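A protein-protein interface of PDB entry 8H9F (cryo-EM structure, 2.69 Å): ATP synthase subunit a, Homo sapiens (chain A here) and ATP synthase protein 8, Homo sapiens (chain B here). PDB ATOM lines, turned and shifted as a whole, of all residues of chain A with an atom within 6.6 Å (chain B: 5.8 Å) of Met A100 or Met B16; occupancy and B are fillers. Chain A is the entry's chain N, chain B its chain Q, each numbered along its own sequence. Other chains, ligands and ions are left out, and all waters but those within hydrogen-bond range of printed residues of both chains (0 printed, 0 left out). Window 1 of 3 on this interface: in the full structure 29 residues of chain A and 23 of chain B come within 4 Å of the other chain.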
ATOM      1  N   ILE A  24      24.108  13.266  18.674  1.00  0.00           N
ATOM      2  CA  ILE A  24      25.385  13.799  18.214  1.00  0.00           C
ATOM      3  C   ILE A  24      26.201  14.355  19.378  1.00  0.00           C
ATOM      4  O   ILE A  24      27.435  14.294  19.354  1.00  0.00           O
ATOM      5  CB  ILE A  24      25.159  14.858  17.122  1.00  0.00           C
ATOM      6  CG1 ILE A  24      24.472  14.235  15.911  1.00  0.00           C
ATOM      7  CG2 ILE A  24      26.470  15.468  16.680  1.00  0.00           C
ATOM      8  CD1 ILE A  24      24.297  15.183  14.756  1.00  0.00           C
ATOM      9  N   LEU A  25      25.550  14.888  20.413  1.00  0.00           N
ATOM     10  CA  LEU A  25      26.290  15.406  21.559  1.00  0.00           C
ATOM     11  C   LEU A  25      26.746  14.316  22.518  1.00  0.00           C
ATOM     12  O   LEU A  25      27.630  14.567  23.340  1.00  0.00           O
ATOM     13  CB  LEU A  25      25.444  16.421  22.325  1.00  0.00           C
ATOM     14  CG  LEU A  25      25.122  17.743  21.630  1.00  0.00           C
ATOM     15  CD1 LEU A  25      23.965  18.420  22.326  1.00  0.00           C
ATOM     16  CD2 LEU A  25      26.327  18.653  21.612  1.00  0.00           C
ATOM     17  N   PHE A  78      36.131  11.527  17.492  1.00  0.00           N
ATOM     18  CA  PHE A  78      34.716  11.852  17.366  1.00  0.00           C
ATOM     19  C   PHE A  78      34.019  10.930  16.378  1.00  0.00           C
ATOM     20  O   PHE A  78      32.889  10.502  16.621  1.00  0.00           O
ATOM     21  CB  PHE A  78      34.539  13.313  16.953  1.00  0.00           C
ATOM     22  CG  PHE A  78      33.189  13.623  16.381  1.00  0.00           C
ATOM     23  CD1 PHE A  78      32.080  13.706  17.197  1.00  0.00           C
ATOM     24  CD2 PHE A  78      33.031  13.840  15.027  1.00  0.00           C
ATOM     25  CE1 PHE A  78      30.840  13.990  16.670  1.00  0.00           C
ATOM     26  CE2 PHE A  78      31.794  14.123  14.501  1.00  0.00           C
ATOM     27  CZ  PHE A  78      30.698  14.198  15.323  1.00  0.00           C
ATOM     28  N   ILE A  79      34.676  10.610  15.265  1.00  0.00           N
ATOM     29  CA  ILE A  79      34.064   9.741  14.266  1.00  0.00           C
ATOM     30  C   ILE A  79      33.975   8.312  14.784  1.00  0.00           C
ATOM     31  O   ILE A  79      32.901   7.701  14.774  1.00  0.00           O
ATOM     32  CB  ILE A  79      34.844   9.815  12.943  1.00  0.00           C
ATOM     33  CG1 ILE A  79      34.877  11.251  12.427  1.00  0.00           C
ATOM     34  CG2 ILE A  79      34.217   8.912  11.909  1.00  0.00           C
ATOM     35  CD1 ILE A  79      35.552  11.403  11.087  1.00  0.00           C
ATOM     36  N   THR A  82      31.353   7.694  17.286  1.00  0.00           N
ATOM     37  CA  THR A  82      30.097   7.906  16.576  1.00  0.00           C
ATOM     38  C   THR A  82      29.778   6.737  15.659  1.00  0.00           C
ATOM     39  O   THR A  82      28.608   6.383  15.485  1.00  0.00           O
ATOM     40  CB  THR A  82      30.160   9.206  15.778  1.00  0.00           C
ATOM     41  OG1 THR A  82      30.328  10.307  16.676  1.00  0.00           O
ATOM     42  CG2 THR A  82      28.894   9.415  14.979  1.00  0.00           C
ATOM     43  N   PRO A  94      24.760   9.278  12.984  1.00  0.00           N
ATOM     44  CA  PRO A  94      24.852  10.530  12.223  1.00  0.00           C
ATOM     45  C   PRO A  94      25.908  10.517  11.133  1.00  0.00           C
ATOM     46  O   PRO A  94      25.851  11.371  10.244  1.00  0.00           O
ATOM     47  CB  PRO A  94      25.167  11.578  13.299  1.00  0.00           C
ATOM     48  CG  PRO A  94      25.625  10.819  14.473  1.00  0.00           C
ATOM     49  CD  PRO A  94      24.962   9.492  14.425  1.00  0.00           C
ATOM     50  N   THR A  95      26.862   9.590  11.159  1.00  0.00           N
ATOM     51  CA  THR A  95      27.825   9.498  10.069  1.00  0.00           C
ATOM     52  C   THR A  95      27.252   8.822   8.832  1.00  0.00           C
ATOM     53  O   THR A  95      27.959   8.705   7.829  1.00  0.00           O
ATOM     54  CB  THR A  95      29.087   8.760  10.520  1.00  0.00           C
ATOM     55  OG1 THR A  95      28.727   7.607  11.285  1.00  0.00           O
ATOM     56  CG2 THR A  95      29.960   9.665  11.359  1.00  0.00           C
ATOM     57  N   THR A  96      26.002   8.368   8.881  1.00  0.00           N
ATOM     58  CA  THR A  96      25.291   7.935   7.689  1.00  0.00           C
ATOM     59  C   THR A  96      24.673   9.098   6.932  1.00  0.00           C
ATOM     60  O   THR A  96      24.111   8.885   5.854  1.00  0.00           O
ATOM     61  CB  THR A  96      24.188   6.936   8.048  1.00  0.00           C
ATOM     62  OG1 THR A  96      23.177   7.595   8.815  1.00  0.00           O
ATOM     63  CG2 THR A  96      24.742   5.791   8.848  1.00  0.00           C
ATOM     64  N   GLN A  97      24.762  10.309   7.468  1.00  0.00           N
ATOM     65  CA  GLN A  97      24.154  11.488   6.872  1.00  0.00           C
ATOM     66  C   GLN A  97      25.192  12.245   6.059  1.00  0.00           C
ATOM     67  O   GLN A  97      26.268  12.569   6.569  1.00  0.00           O
ATOM     68  CB  GLN A  97      23.571  12.398   7.950  1.00  0.00           C
ATOM     69  CG  GLN A  97      22.704  11.684   8.959  1.00  0.00           C
ATOM     70  CD  GLN A  97      21.399  11.224   8.368  1.00  0.00           C
ATOM     71  OE1 GLN A  97      20.553  12.035   8.000  1.00  0.00           O
ATOM     72  NE2 GLN A  97      21.225   9.916   8.269  1.00  0.00           N
ATOM     73  N   LEU A  98      24.867  12.529   4.798  1.00  0.00           N
ATOM     74  CA  LEU A  98      25.749  13.336   3.968  1.00  0.00           C
ATOM     75  C   LEU A  98      25.908  14.745   4.518  1.00  0.00           C
ATOM     76  O   LEU A  98      26.912  15.403   4.231  1.00  0.00           O
ATOM     77  CB  LEU A  98      25.214  13.374   2.535  1.00  0.00           C
ATOM     78  CG  LEU A  98      26.040  14.064   1.448  1.00  0.00           C
ATOM     79  CD1 LEU A  98      27.402  13.420   1.298  1.00  0.00           C
ATOM     80  CD2 LEU A  98      25.290  14.031   0.132  1.00  0.00           C
ATOM     81  N   SER A  99      24.950  15.206   5.321  1.00  0.00           N
ATOM     82  CA  SER A  99      25.016  16.533   5.921  1.00  0.00           C
ATOM     83  C   SER A  99      26.224  16.666   6.838  1.00  0.00           C
ATOM     84  O   SER A  99      27.100  17.514   6.627  1.00  0.00           O
ATOM     85  CB  SER A  99      23.738  16.788   6.709  1.00  0.00           C
ATOM     86  OG  SER A  99      22.611  16.607   5.888  1.00  0.00           O
ATOM     87  N   MET A 100      26.258  15.846   7.889  1.00  0.00           N
ATOM     88  CA  MET A 100      27.333  15.913   8.870  1.00  0.00           C
ATOM     89  C   MET A 100      28.685  15.639   8.228  1.00  0.00           C
ATOM     90  O   MET A 100      29.688  16.267   8.579  1.00  0.00           O
ATOM     91  CB  MET A 100      27.057  14.914   9.992  1.00  0.00           C
ATOM     92  CG  MET A 100      27.498  15.369  11.357  1.00  0.00           C
ATOM     93  SD  MET A 100      27.592  14.010  12.526  1.00  0.00           S
ATOM     94  CE  MET A 100      29.052  13.175  11.934  1.00  0.00           C
ATOM     95  N   ASN A 101      28.729  14.717   7.269  1.00  0.00           N
ATOM     96  CA  ASN A 101      30.001  14.369   6.650  1.00  0.00           C
ATOM     97  C   ASN A 101      30.498  15.484   5.740  1.00  0.00           C
ATOM     98  O   ASN A 101      31.702  15.750   5.683  1.00  0.00           O
ATOM     99  CB  ASN A 101      29.862  13.057   5.889  1.00  0.00           C
ATOM    100  CG  ASN A 101      29.468  11.913   6.790  1.00  0.00           C
ATOM    101  OD1 ASN A 101      29.943  11.808   7.914  1.00  0.00           O
ATOM    102  ND2 ASN A 101      28.587  11.057   6.308  1.00  0.00           N
ATOM    103  N   LEU A 102      29.590  16.163   5.037  1.00  0.00           N
ATOM    104  CA  LEU A 102      29.992  17.335   4.266  1.00  0.00           C
ATOM    105  C   LEU A 102      30.484  18.449   5.181  1.00  0.00           C
ATOM    106  O   LEU A 102      31.490  19.105   4.889  1.00  0.00           O
ATOM    107  CB  LEU A 102      28.829  17.827   3.409  1.00  0.00           C
ATOM    108  CG  LEU A 102      28.689  17.230   2.011  1.00  0.00           C
ATOM    109  CD1 LEU A 102      27.502  17.850   1.308  1.00  0.00           C
ATOM    110  CD2 LEU A 102      29.958  17.432   1.204  1.00  0.00           C
ATOM    111  N   ALA A 103      29.785  18.676   6.294  1.00  0.00           N
ATOM    112  CA  ALA A 103      30.203  19.708   7.236  1.00  0.00           C
ATOM    113  C   ALA A 103      31.500  19.357   7.951  1.00  0.00           C
ATOM    114  O   ALA A 103      32.139  20.244   8.519  1.00  0.00           O
ATOM    115  CB  ALA A 103      29.104  19.960   8.262  1.00  0.00           C
ATOM    116  N   MET A 104      31.879  18.082   7.973  1.00  0.00           N
ATOM    117  CA  MET A 104      33.190  17.719   8.496  1.00  0.00           C
ATOM    118  C   MET A 104      34.269  17.837   7.429  1.00  0.00           C
ATOM    119  O   MET A 104      35.405  18.216   7.731  1.00  0.00           O
ATOM    120  CB  MET A 104      33.164  16.297   9.052  1.00  0.00           C
ATOM    121  CG  MET A 104      32.552  16.167  10.423  1.00  0.00           C
ATOM    122  SD  MET A 104      32.956  14.591  11.186  1.00  0.00           S
ATOM    123  CE  MET A 104      32.253  13.464   9.995  1.00  0.00           C
ATOM    124  N   ALA A 105      33.933  17.524   6.177  1.00  0.00           N
ATOM    125  CA  ALA A 105      34.947  17.428   5.136  1.00  0.00           C
ATOM    126  C   ALA A 105      35.296  18.784   4.536  1.00  0.00           C
ATOM    127  O   ALA A 105      36.478  19.087   4.342  1.00  0.00           O
ATOM    128  CB  ALA A 105      34.480  16.473   4.040  1.00  0.00           C
ATOM    129  N   ALA A 157      33.545  13.009   2.192  1.00  0.00           N
ATOM    130  CA  ALA A 157      32.207  12.921   2.764  1.00  0.00           C
ATOM    131  C   ALA A 157      31.444  11.728   2.211  1.00  0.00           C
ATOM    132  O   ALA A 157      30.802  10.990   2.967  1.00  0.00           O
ATOM    133  CB  ALA A 157      31.441  14.215   2.498  1.00  0.00           C
ATOM    134  N   LEU A 160      32.797   8.281   3.582  1.00  0.00           N
ATOM    135  CA  LEU A 160      32.299   7.971   4.921  1.00  0.00           C
ATOM    136  C   LEU A 160      30.811   7.627   4.892  1.00  0.00           C
ATOM    137  O   LEU A 160      30.388   6.582   5.414  1.00  0.00           O
ATOM    138  CB  LEU A 160      32.573   9.143   5.862  1.00  0.00           C
ATOM    139  CG  LEU A 160      32.271   8.931   7.345  1.00  0.00           C
ATOM    140  CD1 LEU A 160      32.914   7.661   7.850  1.00  0.00           C
ATOM    141  CD2 LEU A 160      32.742  10.117   8.150  1.00  0.00           C
ATOM    142  N   THR A 161      30.004   8.490   4.269  1.00  0.00           N
ATOM    143  CA  THR A 161      28.556   8.303   4.246  1.00  0.00           C
ATOM    144  C   THR A 161      28.178   6.978   3.603  1.00  0.00           C
ATOM    145  O   THR A 161      27.441   6.176   4.187  1.00  0.00           O
ATOM    146  CB  THR A 161      27.896   9.459   3.494  1.00  0.00           C
ATOM    147  OG1 THR A 161      28.268  10.701   4.096  1.00  0.00           O
ATOM    148  CG2 THR A 161      26.390   9.320   3.527  1.00  0.00           C
ATOM    149  N   PHE A 214      39.276   8.702   7.135  1.00  0.00           N
ATOM    150  CA  PHE A 214      38.871  10.103   7.062  1.00  0.00           C
ATOM    151  C   PHE A 214      39.939  11.001   7.670  1.00  0.00           C
ATOM    152  O   PHE A 214      40.398  11.968   7.039  1.00  0.00           O
ATOM    153  CB  PHE A 214      37.532  10.287   7.776  1.00  0.00           C
ATOM    154  CG  PHE A 214      36.850  11.596   7.487  1.00  0.00           C
ATOM    155  CD1 PHE A 214      37.253  12.759   8.113  1.00  0.00           C
ATOM    156  CD2 PHE A 214      35.784  11.655   6.612  1.00  0.00           C
ATOM    157  CE1 PHE A 214      36.621  13.951   7.858  1.00  0.00           C
ATOM    158  CE2 PHE A 214      35.149  12.847   6.360  1.00  0.00           C
ATOM    159  CZ  PHE A 214      35.568  13.992   6.982  1.00  0.00           C
ATOM    160  N   MET B  12      21.518  18.453  11.760  1.00  0.00           N
ATOM    161  CA  MET B  12      22.686  17.585  11.729  1.00  0.00           C
ATOM    162  C   MET B  12      23.998  18.353  11.728  1.00  0.00           C
ATOM    163  O   MET B  12      25.021  17.809  12.154  1.00  0.00           O
ATOM    164  CB  MET B  12      22.643  16.678  10.500  1.00  0.00           C
ATOM    165  CG  MET B  12      21.405  15.822  10.405  1.00  0.00           C
ATOM    166  SD  MET B  12      21.289  14.642  11.750  1.00  0.00           S
ATOM    167  CE  MET B  12      19.591  14.131  11.563  1.00  0.00           C
ATOM    168  N   ILE B  13      24.000  19.599  11.257  1.00  0.00           N
ATOM    169  CA  ILE B  13      25.246  20.353  11.188  1.00  0.00           C
ATOM    170  C   ILE B  13      25.566  20.989  12.531  1.00  0.00           C
ATOM    171  O   ILE B  13      26.713  20.966  12.987  1.00  0.00           O
ATOM    172  CB  ILE B  13      25.180  21.422  10.081  1.00  0.00           C
ATOM    173  CG1 ILE B  13      24.653  20.839   8.774  1.00  0.00           C
ATOM    174  CG2 ILE B  13      26.546  22.032   9.861  1.00  0.00           C
ATOM    175  CD1 ILE B  13      25.533  19.810   8.175  1.00  0.00           C
ATOM    176  N   THR B  14      24.555  21.562  13.187  1.00  0.00           N
ATOM    177  CA  THR B  14      24.834  22.469  14.298  1.00  0.00           C
ATOM    178  C   THR B  14      25.381  21.751  15.526  1.00  0.00           C
ATOM    179  O   THR B  14      26.387  22.222  16.085  1.00  0.00           O
ATOM    180  CB  THR B  14      23.585  23.290  14.622  1.00  0.00           C
ATOM    181  OG1 THR B  14      23.177  24.010  13.454  1.00  0.00           O
ATOM    182  CG2 THR B  14      23.879  24.281  15.728  1.00  0.00           C
ATOM    183  N   PRO B  15      24.799  20.645  16.007  1.00  0.00           N
ATOM    184  CA  PRO B  15      25.417  19.963  17.154  1.00  0.00           C
ATOM    185  C   PRO B  15      26.800  19.415  16.859  1.00  0.00           C
ATOM    186  O   PRO B  15      27.672  19.473  17.733  1.00  0.00           O
ATOM    187  CB  PRO B  15      24.420  18.842  17.477  1.00  0.00           C
ATOM    188  CG  PRO B  15      23.612  18.683  16.264  1.00  0.00           C
ATOM    189  CD  PRO B  15      23.501  20.039  15.674  1.00  0.00           C
ATOM    190  N   MET B  16      27.034  18.893  15.652  1.00  0.00           N
ATOM    191  CA  MET B  16      28.356  18.379  15.312  1.00  0.00           C
ATOM    192  C   MET B  16      29.425  19.448  15.472  1.00  0.00           C
ATOM    193  O   MET B  16      30.497  19.182  16.026  1.00  0.00           O
ATOM    194  CB  MET B  16      28.364  17.836  13.887  1.00  0.00           C
ATOM    195  CG  MET B  16      29.652  17.128  13.502  1.00  0.00           C
ATOM    196  SD  MET B  16      30.931  18.212  12.848  1.00  0.00           S
ATOM    197  CE  MET B  16      30.005  19.093  11.608  1.00  0.00           C
ATOM    198  N   LEU B  17      29.154  20.662  14.991  1.00  0.00           N
ATOM    199  CA  LEU B  17      30.123  21.743  15.123  1.00  0.00           C
ATOM    200  C   LEU B  17      30.402  22.046  16.587  1.00  0.00           C
ATOM    201  O   LEU B  17      31.506  22.465  16.947  1.00  0.00           O
ATOM    202  CB  LEU B  17      29.622  22.989  14.396  1.00  0.00           C
ATOM    203  CG  LEU B  17      29.346  22.856  12.900  1.00  0.00           C
ATOM    204  CD1 LEU B  17      28.518  24.024  12.414  1.00  0.00           C
ATOM    205  CD2 LEU B  17      30.635  22.757  12.116  1.00  0.00           C
ATOM    206  N   LEU B  18      29.410  21.836  17.453  1.00  0.00           N
ATOM    207  CA  LEU B  18      29.647  22.014  18.878  1.00  0.00           C
ATOM    208  C   LEU B  18      30.343  20.805  19.476  1.00  0.00           C
ATOM    209  O   LEU B  18      31.062  20.929  20.471  1.00  0.00           O
ATOM    210  CB  LEU B  18      28.332  22.280  19.603  1.00  0.00           C
ATOM    211  CG  LEU B  18      27.689  23.627  19.292  1.00  0.00           C
ATOM    212  CD1 LEU B  18      26.206  23.598  19.607  1.00  0.00           C
ATOM    213  CD2 LEU B  18      28.383  24.729  20.066  1.00  0.00           C
ATOM    214  N   THR B  19      30.145  19.630  18.884  1.00  0.00           N
ATOM    215  CA  THR B  19      30.715  18.408  19.433  1.00  0.00           C
ATOM    216  C   THR B  19      32.136  18.183  18.940  1.00  0.00           C
ATOM    217  O   THR B  19      33.014  17.796  19.719  1.00  0.00           O
ATOM    218  CB  THR B  19      29.829  17.223  19.066  1.00  0.00           C
ATOM    219  OG1 THR B  19      28.555  17.372  19.696  1.00  0.00           O
ATOM    220  CG2 THR B  19      30.454  15.936  19.517  1.00  0.00           C
ATOM    221  N   LEU B  20      32.383  18.428  17.656  1.00  0.00           N
ATOM    222  CA  LEU B  20      33.703  18.183  17.096  1.00  0.00           C
ATOM    223  C   LEU B  20      34.674  19.314  17.392  1.00  0.00           C
ATOM    224  O   LEU B  20      35.857  19.058  17.629  1.00  0.00           O
ATOM    225  CB  LEU B  20      33.598  17.967  15.588  1.00  0.00           C
ATOM    226  CG  LEU B  20      34.916  17.886  14.824  1.00  0.00           C
ATOM    227  CD1 LEU B  20      35.714  16.692  15.286  1.00  0.00           C
ATOM    228  CD2 LEU B  20      34.661  17.817  13.334  1.00  0.00           C
ATOM    229  N   PHE B  21      34.205  20.559  17.394  1.00  0.00           N
ATOM    230  CA  PHE B  21      35.094  21.704  17.511  1.00  0.00           C
ATOM    231  C   PHE B  21      35.148  22.301  18.908  1.00  0.00           C
ATOM    232  O   PHE B  21      36.048  23.099  19.180  1.00  0.00           O
ATOM    233  CB  PHE B  21      34.689  22.794  16.515  1.00  0.00           C
ATOM    234  CG  PHE B  21      35.096  22.500  15.103  1.00  0.00           C
ATOM    235  CD1 PHE B  21      36.381  22.761  14.673  1.00  0.00           C
ATOM    236  CD2 PHE B  21      34.197  21.952  14.210  1.00  0.00           C
ATOM    237  CE1 PHE B  21      36.757  22.485  13.379  1.00  0.00           C
ATOM    238  CE2 PHE B  21      34.570  21.674  12.917  1.00  0.00           C
ATOM    239  CZ  PHE B  21      35.850  21.940  12.501  1.00  0.00           C
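O of Ile A24 lies within hydrogen-bond range of OG1 of Thr B19 (3.3 Å).
Printed residues of chain A that touch a printed residue of chain B: Ile A24, Leu A25, Phe A78, Ser A99, Met A100, Ala A103 and Met A104. Hydrophobic or aromatic side chains of chain A that line the printed part of chain B: Ile A24, Leu A25, Phe A78, Met A100, Ala A103 and Met A104. Printed residues of chain B that touch a printed residue of chain A: Met B12, Ile B13, Pro B15, Met B16, Thr B19 and Leu B20.
O of Pro B15 is in hydrogen-bond range of OG1 of Thr B19 (3.0 Å). O of Phe A78 sits at hydrogen-bond distance from OG1 of Thr A82, 2.6 Å away.
CD1 of Ile A24 touches O of Met B12, 3.8 Å away. Pro B15 touches Ile A24. Met B16 touches Ile A24. Phe A78 touches Met B16. CG2 of Thr B19 touches CE1 of Phe A78, at 3.5 Å. Ser A99 touches Ile B13 (O to CD1, 3.2 Å). Met A100 touches Met B16 (CG to CG, 3.5 Å). Ala A103 touches Ile B13. Met B16 touches Met A104 (SD to CG, 3.6 Å). Met A104 touches Leu B20.
Met A100 touches just these residues of chain B: Met B12 (3.6 Å) and Met B16 (3.5 Å). Ala A105 touches none of the printed residues of chain B. Of the printed residues of chain A, Thr B19 touches Ile A24 (3.3 Å), Leu A25 (3.2 Å) and Phe A78 (3.5 Å). Of the printed residues of chain A, Leu B20 touches Phe A78 and Met A104. The nearest printed residue of chain A that does not touch Met B16 is Ser A99 (6.0 Å). The nearest printed residue of chain A that does not touch Thr B19 is Thr A82 (6.3 Å).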
